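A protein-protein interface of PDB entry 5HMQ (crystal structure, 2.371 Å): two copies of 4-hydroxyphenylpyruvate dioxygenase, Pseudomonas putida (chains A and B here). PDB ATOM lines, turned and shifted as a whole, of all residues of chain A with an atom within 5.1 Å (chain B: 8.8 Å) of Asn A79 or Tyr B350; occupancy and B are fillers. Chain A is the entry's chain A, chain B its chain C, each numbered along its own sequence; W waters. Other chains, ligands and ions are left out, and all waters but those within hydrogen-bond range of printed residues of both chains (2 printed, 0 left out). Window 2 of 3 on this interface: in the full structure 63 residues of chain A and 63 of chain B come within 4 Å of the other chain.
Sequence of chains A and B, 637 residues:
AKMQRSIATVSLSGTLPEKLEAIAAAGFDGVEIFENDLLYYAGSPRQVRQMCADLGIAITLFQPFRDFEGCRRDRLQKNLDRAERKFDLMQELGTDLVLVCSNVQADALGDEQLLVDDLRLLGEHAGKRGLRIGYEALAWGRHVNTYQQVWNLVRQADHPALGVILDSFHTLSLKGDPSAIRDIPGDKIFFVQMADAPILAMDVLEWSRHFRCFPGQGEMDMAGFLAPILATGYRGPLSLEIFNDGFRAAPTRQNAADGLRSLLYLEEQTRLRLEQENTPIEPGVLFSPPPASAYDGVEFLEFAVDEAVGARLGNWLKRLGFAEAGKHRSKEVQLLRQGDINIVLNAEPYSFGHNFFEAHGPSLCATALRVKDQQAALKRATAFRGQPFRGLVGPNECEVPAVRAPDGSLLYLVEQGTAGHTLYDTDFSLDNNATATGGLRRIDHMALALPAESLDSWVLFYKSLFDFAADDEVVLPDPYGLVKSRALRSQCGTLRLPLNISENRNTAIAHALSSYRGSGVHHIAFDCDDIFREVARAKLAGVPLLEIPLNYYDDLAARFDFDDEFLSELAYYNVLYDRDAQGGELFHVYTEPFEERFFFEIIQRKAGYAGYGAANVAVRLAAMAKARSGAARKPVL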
ATOM      1  N   PHE A  65      25.426   1.374   6.162  1.00  0.00           N
ATOM      2  CA  PHE A  65      24.771   2.675   6.067  1.00  0.00           C
ATOM      3  C   PHE A  65      24.408   2.897   4.605  1.00  0.00           C
ATOM      4  O   PHE A  65      25.295   3.089   3.766  1.00  0.00           O
ATOM      5  CB  PHE A  65      25.673   3.788   6.594  1.00  0.00           C
ATOM      6  CG  PHE A  65      24.959   5.090   6.809  1.00  0.00           C
ATOM      7  CD1 PHE A  65      24.398   5.386   8.039  1.00  0.00           C
ATOM      8  CD2 PHE A  65      24.830   6.005   5.781  1.00  0.00           C
ATOM      9  CE1 PHE A  65      23.730   6.576   8.242  1.00  0.00           C
ATOM     10  CE2 PHE A  65      24.162   7.200   5.981  1.00  0.00           C
ATOM     11  CZ  PHE A  65      23.613   7.483   7.212  1.00  0.00           C
ATOM     12  N   ARG A  66      23.116   2.857   4.294  1.00  0.00           N
ATOM     13  CA  ARG A  66      22.663   2.822   2.913  1.00  0.00           C
ATOM     14  C   ARG A  66      22.199   4.177   2.398  1.00  0.00           C
ATOM     15  O   ARG A  66      21.768   5.049   3.158  1.00  0.00           O
ATOM     16  CB  ARG A  66      21.537   1.803   2.714  1.00  0.00           C
ATOM     17  CG  ARG A  66      21.955   0.357   2.861  1.00  0.00           C
ATOM     18  CD  ARG A  66      20.757  -0.571   2.767  1.00  0.00           C
ATOM     19  NE  ARG A  66      21.162  -1.974   2.815  1.00  0.00           N
ATOM     20  CZ  ARG A  66      21.157  -2.736   3.899  1.00  0.00           C
ATOM     21  NH1 ARG A  66      20.759  -2.242   5.064  1.00  0.00           N
ATOM     22  NH2 ARG A  66      21.550  -4.000   3.809  1.00  0.00           N
ATOM     23  N   ASP A  67      22.307   4.326   1.073  1.00  0.00           N
ATOM     24  CA  ASP A  67      21.731   5.414   0.289  1.00  0.00           C
ATOM     25  C   ASP A  67      21.933   6.789   0.910  1.00  0.00           C
ATOM     26  O   ASP A  67      20.987   7.381   1.439  1.00  0.00           O
ATOM     27  CB  ASP A  67      20.238   5.154   0.073  1.00  0.00           C
ATOM     28  CG  ASP A  67      19.958   3.749  -0.435  1.00  0.00           C
ATOM     29  OD1 ASP A  67      20.764   3.229  -1.239  1.00  0.00           O
ATOM     30  OD2 ASP A  67      18.935   3.163  -0.024  1.00  0.00           O
ATOM     31  N   PHE A  68      23.158   7.309   0.851  1.00  0.00           N
ATOM     32  CA  PHE A  68      23.442   8.663   1.312  1.00  0.00           C
ATOM     33  C   PHE A  68      23.739   9.599   0.146  1.00  0.00           C
ATOM     34  O   PHE A  68      22.993  10.553  -0.082  1.00  0.00           O
ATOM     35  CB  PHE A  68      24.596   8.670   2.311  1.00  0.00           C
ATOM     36  CG  PHE A  68      24.946  10.040   2.791  1.00  0.00           C
ATOM     37  CD1 PHE A  68      24.235  10.622   3.826  1.00  0.00           C
ATOM     38  CD2 PHE A  68      25.961  10.762   2.188  1.00  0.00           C
ATOM     39  CE1 PHE A  68      24.539  11.889   4.261  1.00  0.00           C
ATOM     40  CE2 PHE A  68      26.268  12.032   2.618  1.00  0.00           C
ATOM     41  CZ  PHE A  68      25.559  12.595   3.655  1.00  0.00           C
ATOM     42  N   CYS A  71      21.228  11.419  -2.965  1.00  0.00           N
ATOM     43  CA  CYS A  71      19.794  11.388  -2.772  1.00  0.00           C
ATOM     44  C   CYS A  71      19.243  12.789  -2.981  1.00  0.00           C
ATOM     45  O   CYS A  71      19.986  13.773  -3.046  1.00  0.00           O
ATOM     46  CB  CYS A  71      19.433  10.855  -1.386  1.00  0.00           C
ATOM     47  SG  CYS A  71      19.175   9.064  -1.343  1.00  0.00           S
ATOM     48  N   ARG A  75      16.136  15.396   1.564  1.00  0.00           N
ATOM     49  CA  ARG A  75      16.427  14.319   2.497  1.00  0.00           C
ATOM     50  C   ARG A  75      17.882  14.331   2.946  1.00  0.00           C
ATOM     51  O   ARG A  75      18.308  13.421   3.666  1.00  0.00           O
ATOM     52  CB  ARG A  75      16.071  12.969   1.869  1.00  0.00           C
ATOM     53  CG  ARG A  75      14.575  12.775   1.646  1.00  0.00           C
ATOM     54  CD  ARG A  75      13.808  12.962   2.948  1.00  0.00           C
ATOM     55  NE  ARG A  75      12.369  12.742   2.804  1.00  0.00           N
ATOM     56  CZ  ARG A  75      11.460  13.713   2.749  1.00  0.00           C
ATOM     57  NH1 ARG A  75      11.834  14.983   2.814  1.00  0.00           N
ATOM     58  NH2 ARG A  75      10.174  13.412   2.618  1.00  0.00           N
ATOM     59  N   LEU A  76      18.653  15.345   2.544  1.00  0.00           N
ATOM     60  CA  LEU A  76      20.062  15.400   2.922  1.00  0.00           C
ATOM     61  C   LEU A  76      20.215  15.650   4.417  1.00  0.00           C
ATOM     62  O   LEU A  76      20.998  14.971   5.091  1.00  0.00           O
ATOM     63  CB  LEU A  76      20.788  16.474   2.110  1.00  0.00           C
ATOM     64  CG  LEU A  76      22.290  16.587   2.387  1.00  0.00           C
ATOM     65  CD1 LEU A  76      22.995  15.273   2.064  1.00  0.00           C
ATOM     66  CD2 LEU A  76      22.903  17.730   1.593  1.00  0.00           C
ATOM     67  N   GLN A  77      19.473  16.618   4.961  1.00  0.00           N
ATOM     68  CA  GLN A  77      19.562  16.863   6.396  1.00  0.00           C
ATOM     69  C   GLN A  77      19.098  15.641   7.173  1.00  0.00           C
ATOM     70  O   GLN A  77      19.797  15.165   8.075  1.00  0.00           O
ATOM     71  CB  GLN A  77      18.746  18.096   6.789  1.00  0.00           C
ATOM     72  CG  GLN A  77      18.835  18.445   8.277  1.00  0.00           C
ATOM     73  CD  GLN A  77      20.245  18.790   8.732  1.00  0.00           C
ATOM     74  OE1 GLN A  77      21.082  19.217   7.937  1.00  0.00           O
ATOM     75  NE2 GLN A  77      20.510  18.606  10.024  1.00  0.00           N
ATOM     76  N   LYS A  78      17.942  15.087   6.795  1.00  0.00           N
ATOM     77  CA  LYS A  78      17.461  13.870   7.442  1.00  0.00           C
ATOM     78  C   LYS A  78      18.487  12.745   7.358  1.00  0.00           C
ATOM     79  O   LYS A  78      18.655  11.976   8.314  1.00  0.00           O
ATOM     80  CB  LYS A  78      16.131  13.437   6.824  1.00  0.00           C
ATOM     81  CG  LYS A  78      14.936  13.666   7.733  1.00  0.00           C
ATOM     82  CD  LYS A  78      13.636  13.310   7.035  1.00  0.00           C
ATOM     83  CE  LYS A  78      13.699  11.914   6.438  1.00  0.00           C
ATOM     84  NZ  LYS A  78      12.396  11.504   5.846  1.00  0.00           N
ATOM     85  N   ASN A  79      19.192  12.634   6.228  1.00  0.00           N
ATOM     86  CA  ASN A  79      20.233  11.612   6.116  1.00  0.00           C
ATOM     87  C   ASN A  79      21.423  11.894   7.026  1.00  0.00           C
ATOM     88  O   ASN A  79      22.061  10.951   7.504  1.00  0.00           O
ATOM     89  CB  ASN A  79      20.707  11.480   4.667  1.00  0.00           C
ATOM     90  CG  ASN A  79      19.817  10.575   3.847  1.00  0.00           C
ATOM     91  OD1 ASN A  79      19.310   9.573   4.344  1.00  0.00           O
ATOM     92  ND2 ASN A  79      19.637  10.915   2.573  1.00  0.00           N
ATOM     93  N   LEU A  80      21.754  13.172   7.256  1.00  0.00           N
ATOM     94  CA  LEU A  80      22.837  13.483   8.178  1.00  0.00           C
ATOM     95  C   LEU A  80      22.444  13.193   9.620  1.00  0.00           C
ATOM     96  O   LEU A  80      23.272  12.727  10.407  1.00  0.00           O
ATOM     97  CB  LEU A  80      23.275  14.946   8.026  1.00  0.00           C
ATOM     98  CG  LEU A  80      23.874  15.295   6.654  1.00  0.00           C
ATOM     99  CD1 LEU A  80      24.070  16.805   6.521  1.00  0.00           C
ATOM    100  CD2 LEU A  80      25.178  14.531   6.425  1.00  0.00           C
ATOM    101  N   ASP A  81      21.194  13.481   9.994  1.00  0.00           N
ATOM    102  CA  ASP A  81      20.710  13.103  11.322  1.00  0.00           C
ATOM    103  C   ASP A  81      20.781  11.594  11.520  1.00  0.00           C
ATOM    104  O   ASP A  81      21.112  11.114  12.610  1.00  0.00           O
ATOM    105  CB  ASP A  81      19.268  13.588  11.521  1.00  0.00           C
ATOM    106  CG  ASP A  81      19.148  15.100  11.528  1.00  0.00           C
ATOM    107  OD1 ASP A  81      19.369  15.728  10.480  1.00  0.00           O
ATOM    108  OD2 ASP A  81      18.828  15.668  12.592  1.00  0.00           O
ATOM    109  N   ARG A  82      20.463  10.829  10.473  1.00  0.00           N
ATOM    110  CA  ARG A  82      20.604   9.377  10.543  1.00  0.00           C
ATOM    111  C   ARG A  82      22.064   8.989  10.730  1.00  0.00           C
ATOM    112  O   ARG A  82      22.381   8.079  11.506  1.00  0.00           O
ATOM    113  CB  ARG A  82      20.023   8.737   9.279  1.00  0.00           C
ATOM    114  CG  ARG A  82      20.169   7.223   9.206  1.00  0.00           C
ATOM    115  CD  ARG A  82      19.317   6.621   8.090  1.00  0.00           C
ATOM    116  NE  ARG A  82      19.686   7.101   6.759  1.00  0.00           N
ATOM    117  CZ  ARG A  82      20.428   6.413   5.894  1.00  0.00           C
ATOM    118  NH1 ARG A  82      20.882   5.209   6.217  1.00  0.00           N
ATOM    119  NH2 ARG A  82      20.713   6.924   4.705  1.00  0.00           N
ATOM    120  N   ALA A  83      22.971   9.680  10.032  1.00  0.00           N
ATOM    121  CA  ALA A  83      24.397   9.439  10.226  1.00  0.00           C
ATOM    122  C   ALA A  83      24.819   9.755  11.654  1.00  0.00           C
ATOM    123  O   ALA A  83      25.626   9.030  12.247  1.00  0.00           O
ATOM    124  CB  ALA A  83      25.210  10.261   9.225  1.00  0.00           C
ATOM    125  N   VAL B 305       9.129  -4.732   1.310  1.00  0.00           N
ATOM    126  CA  VAL B 305       9.282  -4.316  -0.079  1.00  0.00           C
ATOM    127  C   VAL B 305       9.935  -2.941  -0.104  1.00  0.00           C
ATOM    128  O   VAL B 305      10.030  -2.255   0.914  1.00  0.00           O
ATOM    129  CB  VAL B 305       7.927  -4.262  -0.826  1.00  0.00           C
ATOM    130  CG1 VAL B 305       7.381  -5.658  -1.087  1.00  0.00           C
ATOM    131  CG2 VAL B 305       6.924  -3.435  -0.033  1.00  0.00           C
ATOM    132  N   LYS B 331       4.842   6.809   7.945  1.00  0.00           N
ATOM    133  CA  LYS B 331       5.760   5.894   7.284  1.00  0.00           C
ATOM    134  C   LYS B 331       5.267   5.529   5.887  1.00  0.00           C
ATOM    135  O   LYS B 331       4.106   5.747   5.530  1.00  0.00           O
ATOM    136  CB  LYS B 331       5.950   4.626   8.120  1.00  0.00           C
ATOM    137  CG  LYS B 331       6.423   4.892   9.538  1.00  0.00           C
ATOM    138  CD  LYS B 331       6.398   3.626  10.373  1.00  0.00           C
ATOM    139  CE  LYS B 331       7.017   3.860  11.739  1.00  0.00           C
ATOM    140  NZ  LYS B 331       6.952   2.637  12.586  1.00  0.00           N
ATOM    141  N   ASN B 346       5.042  -2.846   3.582  1.00  0.00           N
ATOM    142  CA  ASN B 346       5.987  -2.063   4.374  1.00  0.00           C
ATOM    143  C   ASN B 346       7.173  -1.702   3.483  1.00  0.00           C
ATOM    144  O   ASN B 346       8.022  -2.545   3.185  1.00  0.00           O
ATOM    145  CB  ASN B 346       6.415  -2.852   5.608  1.00  0.00           C
ATOM    146  CG  ASN B 346       7.331  -2.065   6.530  1.00  0.00           C
ATOM    147  OD1 ASN B 346       7.669  -0.912   6.262  1.00  0.00           O
ATOM    148  ND2 ASN B 346       7.719  -2.684   7.638  1.00  0.00           N
ATOM    149  N   ALA B 347       7.220  -0.442   3.049  1.00  0.00           N
ATOM    150  CA  ALA B 347       8.323   0.073   2.250  1.00  0.00           C
ATOM    151  C   ALA B 347       9.152   1.109   2.998  1.00  0.00           C
ATOM    152  O   ALA B 347       9.963   1.806   2.379  1.00  0.00           O
ATOM    153  CB  ALA B 347       7.798   0.669   0.941  1.00  0.00           C
ATOM    154  N   GLU B 348       8.965   1.229   4.306  1.00  0.00           N
ATOM    155  CA  GLU B 348       9.716   2.194   5.102  1.00  0.00           C
ATOM    156  C   GLU B 348      11.180   1.778   5.189  1.00  0.00           C
ATOM    157  O   GLU B 348      11.472   0.670   5.656  1.00  0.00           O
ATOM    158  CB  GLU B 348       9.111   2.313   6.497  1.00  0.00           C
ATOM    159  CG  GLU B 348       9.835   3.279   7.429  1.00  0.00           C
ATOM    160  CD  GLU B 348       9.567   4.742   7.109  1.00  0.00           C
ATOM    161  OE1 GLU B 348       8.924   5.034   6.077  1.00  0.00           O
ATOM    162  OE2 GLU B 348       9.998   5.607   7.901  1.00  0.00           O
ATOM    163  N   PRO B 349      12.118   2.615   4.763  1.00  0.00           N
ATOM    164  CA  PRO B 349      13.534   2.243   4.824  1.00  0.00           C
ATOM    165  C   PRO B 349      14.104   2.400   6.230  1.00  0.00           C
ATOM    166  O   PRO B 349      13.506   3.014   7.114  1.00  0.00           O
ATOM    167  CB  PRO B 349      14.191   3.221   3.845  1.00  0.00           C
ATOM    168  CG  PRO B 349      13.328   4.435   3.918  1.00  0.00           C
ATOM    169  CD  PRO B 349      11.920   3.939   4.147  1.00  0.00           C
ATOM    170  N   TYR B 350      15.293   1.819   6.411  1.00  0.00           N
ATOM    171  CA  TYR B 350      16.075   1.921   7.644  1.00  0.00           C
ATOM    172  C   TYR B 350      15.262   1.412   8.833  1.00  0.00           C
ATOM    173  O   TYR B 350      14.992   2.133   9.795  1.00  0.00           O
ATOM    174  CB  TYR B 350      16.537   3.361   7.884  1.00  0.00           C
ATOM    175  CG  TYR B 350      16.844   4.125   6.626  1.00  0.00           C
ATOM    176  CD1 TYR B 350      16.221   5.337   6.372  1.00  0.00           C
ATOM    177  CD2 TYR B 350      17.694   3.608   5.655  1.00  0.00           C
ATOM    178  CE1 TYR B 350      16.467   6.037   5.220  1.00  0.00           C
ATOM    179  CE2 TYR B 350      17.947   4.303   4.493  1.00  0.00           C
ATOM    180  CZ  TYR B 350      17.329   5.517   4.282  1.00  0.00           C
ATOM    181  OH  TYR B 350      17.573   6.218   3.126  1.00  0.00           O
ATOM    182  N   SER B 351      14.883   0.144   8.752  1.00  0.00           N
ATOM    183  CA  SER B 351      13.938  -0.420   9.702  1.00  0.00           C
ATOM    184  C   SER B 351      14.054  -1.936   9.666  1.00  0.00           C
ATOM    185  O   SER B 351      14.841  -2.504   8.903  1.00  0.00           O
ATOM    186  CB  SER B 351      12.510   0.037   9.386  1.00  0.00           C
ATOM    187  OG  SER B 351      12.110  -0.412   8.103  1.00  0.00           O
ATOM    188  N   PHE B 352      13.259  -2.587  10.515  1.00  0.00           N
ATOM    189  CA  PHE B 352      13.179  -4.042  10.502  1.00  0.00           C
ATOM    190  C   PHE B 352      12.774  -4.552   9.125  1.00  0.00           C
ATOM    191  O   PHE B 352      13.416  -5.452   8.572  1.00  0.00           O
ATOM    192  CB  PHE B 352      12.200  -4.504  11.583  1.00  0.00           C
ATOM    193  CG  PHE B 352      11.494  -5.786  11.266  1.00  0.00           C
ATOM    194  CD1 PHE B 352      12.136  -7.004  11.408  1.00  0.00           C
ATOM    195  CD2 PHE B 352      10.172  -5.775  10.850  1.00  0.00           C
ATOM    196  CE1 PHE B 352      11.478  -8.185  11.121  1.00  0.00           C
ATOM    197  CE2 PHE B 352       9.509  -6.952  10.562  1.00  0.00           C
ATOM    198  CZ  PHE B 352      10.163  -8.157  10.699  1.00  0.00           C
ATOM    199  N   GLY B 353      11.722  -3.969   8.548  1.00  0.00           N
ATOM    200  CA  GLY B 353      11.280  -4.395   7.229  1.00  0.00           C
ATOM    201  C   GLY B 353      12.330  -4.194   6.152  1.00  0.00           C
ATOM    202  O   GLY B 353      12.530  -5.062   5.298  1.00  0.00           O
ATOM    203  N   HIS B 354      13.019  -3.049   6.178  1.00  0.00           N
ATOM    204  CA  HIS B 354      14.013  -2.761   5.147  1.00  0.00           C
ATOM    205  C   HIS B 354      15.170  -3.751   5.199  1.00  0.00           C
ATOM    206  O   HIS B 354      15.642  -4.218   4.155  1.00  0.00           O
ATOM    207  CB  HIS B 354      14.523  -1.326   5.293  1.00  0.00           C
ATOM    208  CG  HIS B 354      15.422  -0.889   4.178  1.00  0.00           C
ATOM    209  ND1 HIS B 354      16.319   0.149   4.308  1.00  0.00           N
ATOM    210  CD2 HIS B 354      15.560  -1.347   2.910  1.00  0.00           C
ATOM    211  CE1 HIS B 354      16.973   0.310   3.171  1.00  0.00           C
ATOM    212  NE2 HIS B 354      16.531  -0.585   2.306  1.00  0.00           N
ATOM    213  N   ASN B 355      15.650  -4.074   6.401  1.00  0.00           N
ATOM    214  CA  ASN B 355      16.672  -5.108   6.534  1.00  0.00           C
ATOM    215  C   ASN B 355      16.184  -6.431   5.959  1.00  0.00           C
ATOM    216  O   ASN B 355      16.911  -7.109   5.222  1.00  0.00           O
ATOM    217  CB  ASN B 355      17.070  -5.272   8.002  1.00  0.00           C
ATOM    218  CG  ASN B 355      17.810  -4.065   8.546  1.00  0.00           C
ATOM    219  OD1 ASN B 355      18.320  -3.240   7.787  1.00  0.00           O
ATOM    220  ND2 ASN B 355      17.868  -3.953   9.868  1.00  0.00           N
ATOM    221  N   PHE B 356      14.942  -6.807   6.278  1.00  0.00           N
ATOM    222  CA  PHE B 356      14.387  -8.061   5.780  1.00  0.00           C
ATOM    223  C   PHE B 356      14.280  -8.051   4.260  1.00  0.00           C
ATOM    224  O   PHE B 356      14.557  -9.063   3.605  1.00  0.00           O
ATOM    225  CB  PHE B 356      13.019  -8.309   6.415  1.00  0.00           C
ATOM    226  CG  PHE B 356      12.638  -9.758   6.496  1.00  0.00           C
ATOM    227  CD1 PHE B 356      12.013 -10.383   5.430  1.00  0.00           C
ATOM    228  CD2 PHE B 356      12.904 -10.494   7.637  1.00  0.00           C
ATOM    229  CE1 PHE B 356      11.657 -11.716   5.502  1.00  0.00           C
ATOM    230  CE2 PHE B 356      12.554 -11.828   7.715  1.00  0.00           C
ATOM    231  CZ  PHE B 356      11.930 -12.440   6.646  1.00  0.00           C
ATOM    232  N   GLU B 358      16.188  -6.262   2.162  1.00  0.00           N
ATOM    233  CA  GLU B 358      17.534  -6.359   1.609  1.00  0.00           C
ATOM    234  C   GLU B 358      18.106  -7.761   1.782  1.00  0.00           C
ATOM    235  O   GLU B 358      18.870  -8.229   0.930  1.00  0.00           O
ATOM    236  CB  GLU B 358      18.447  -5.324   2.265  1.00  0.00           C
ATOM    237  CG  GLU B 358      18.086  -3.872   1.953  1.00  0.00           C
ATOM    238  CD  GLU B 358      18.211  -3.524   0.479  1.00  0.00           C
ATOM    239  OE1 GLU B 358      19.095  -4.088  -0.201  1.00  0.00           O
ATOM    240  OE2 GLU B 358      17.429  -2.673   0.001  1.00  0.00           O
ATOM    241  N   GLU B 397       7.935  -3.070  15.587  1.00  0.00           N
ATOM    242  CA  GLU B 397       7.468  -1.701  15.443  1.00  0.00           C
ATOM    243  C   GLU B 397       5.964  -1.576  15.644  1.00  0.00           C
ATOM    244  O   GLU B 397       5.401  -0.506  15.394  1.00  0.00           O
ATOM    245  CB  GLU B 397       7.878  -1.147  14.077  1.00  0.00           C
ATOM    246  CG  GLU B 397       9.387  -1.128  13.881  1.00  0.00           C
ATOM    247  CD  GLU B 397       9.814  -0.453  12.595  1.00  0.00           C
ATOM    248  OE1 GLU B 397       8.957   0.179  11.941  1.00  0.00           O
ATOM    249  OE2 GLU B 397      11.010  -0.555  12.240  1.00  0.00           O
HETATM  250  O   HOH W   1      18.767   0.324   0.340  1.00  0.00           O
HETATM  251  O   HOH W   2      20.449  -4.469   6.381  1.00  0.00           O
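Hydrophobic or aromatic side chains of chain B within 4 Å of the printed part of chain A: Tyr B350 and His B354. Of the 14 printed residues of chain A, 4 touch a printed residue of chain B. Among the printed residues, 6 pairs touch across the chains. Among the printed residues, no Asp or Glu carboxylate lies within 4 Å of a Lys or Arg side-chain nitrogen of the other chain.
Water W2 bridges the guanidinium group of Arg A66 and the side-chain amide oxygen of Asn B355. Water W1 lies within hydrogen-bond range of OD2 of Asp A67 (2.9 Å), NE2 of His B354 (3.1 Å) and OE2 of Glu B358 (3.3 Å).
No position is printed for both chains. Of the 6 pairs that touch across the chains among the printed residues, none has its exchanged pair printed and touching as well.
A ring nitrogen (ND1) of His B354 is in hydrogen-bond range of the backbone NH (N) of Tyr B350, 2.9 Å away. The side-chain hydroxyl of Ser B351 is in hydrogen-bond range of the backbone NH of His B354 (3.4 Å). The backbone carbonyl oxygen (O) of Ser B351 lies close to the side-chain amide nitrogen (ND2) of Asn B355 (3.5 Å). O of Arg A75 is in hydrogen-bond range of ND2 of Asn A79 (3.0 Å). O of Asp A67 is in hydrogen-bond range of SG of Cys A71 (3.7 Å). NH2 of Arg A82 is in hydrogen-bond range of O of Asp A67 (3.3 Å).
Asn A79 touches just one residue of chain B: Tyr B350. Of the printed residues of chain A, Tyr B350 touches Asp A67, Asn A79 and Arg A82. Printed residues of chain B within 4 Å of Arg A82: Tyr B350. Printed residues of chain A within 4 Å of His B354: Arg A66. Of the printed residues of chain A, Glu B358 touches Arg A66. Of the printed residues of chain B, Asp A67 touches Tyr B350 (3.98 Å). Asp A81 touches none of the printed residues of chain B. Leu A80 touches none of the printed residues of chain B. The nearest printed residue of chain A that does not touch Tyr B350 is Arg A66 (4.1 Å).
Among the printed residues, pairs that only touch across the chains: Arg A82 with Tyr B350 (3.5 Å), Arg A66 with Glu B358 (3.7 Å), Arg A66 with Asn B355 (3.8 Å), Arg A66 with His B354 (3.9 Å), Asn A79 with Tyr B350 (3.97 Å) and Asp A67 with Tyr B350 (3.98 Å).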
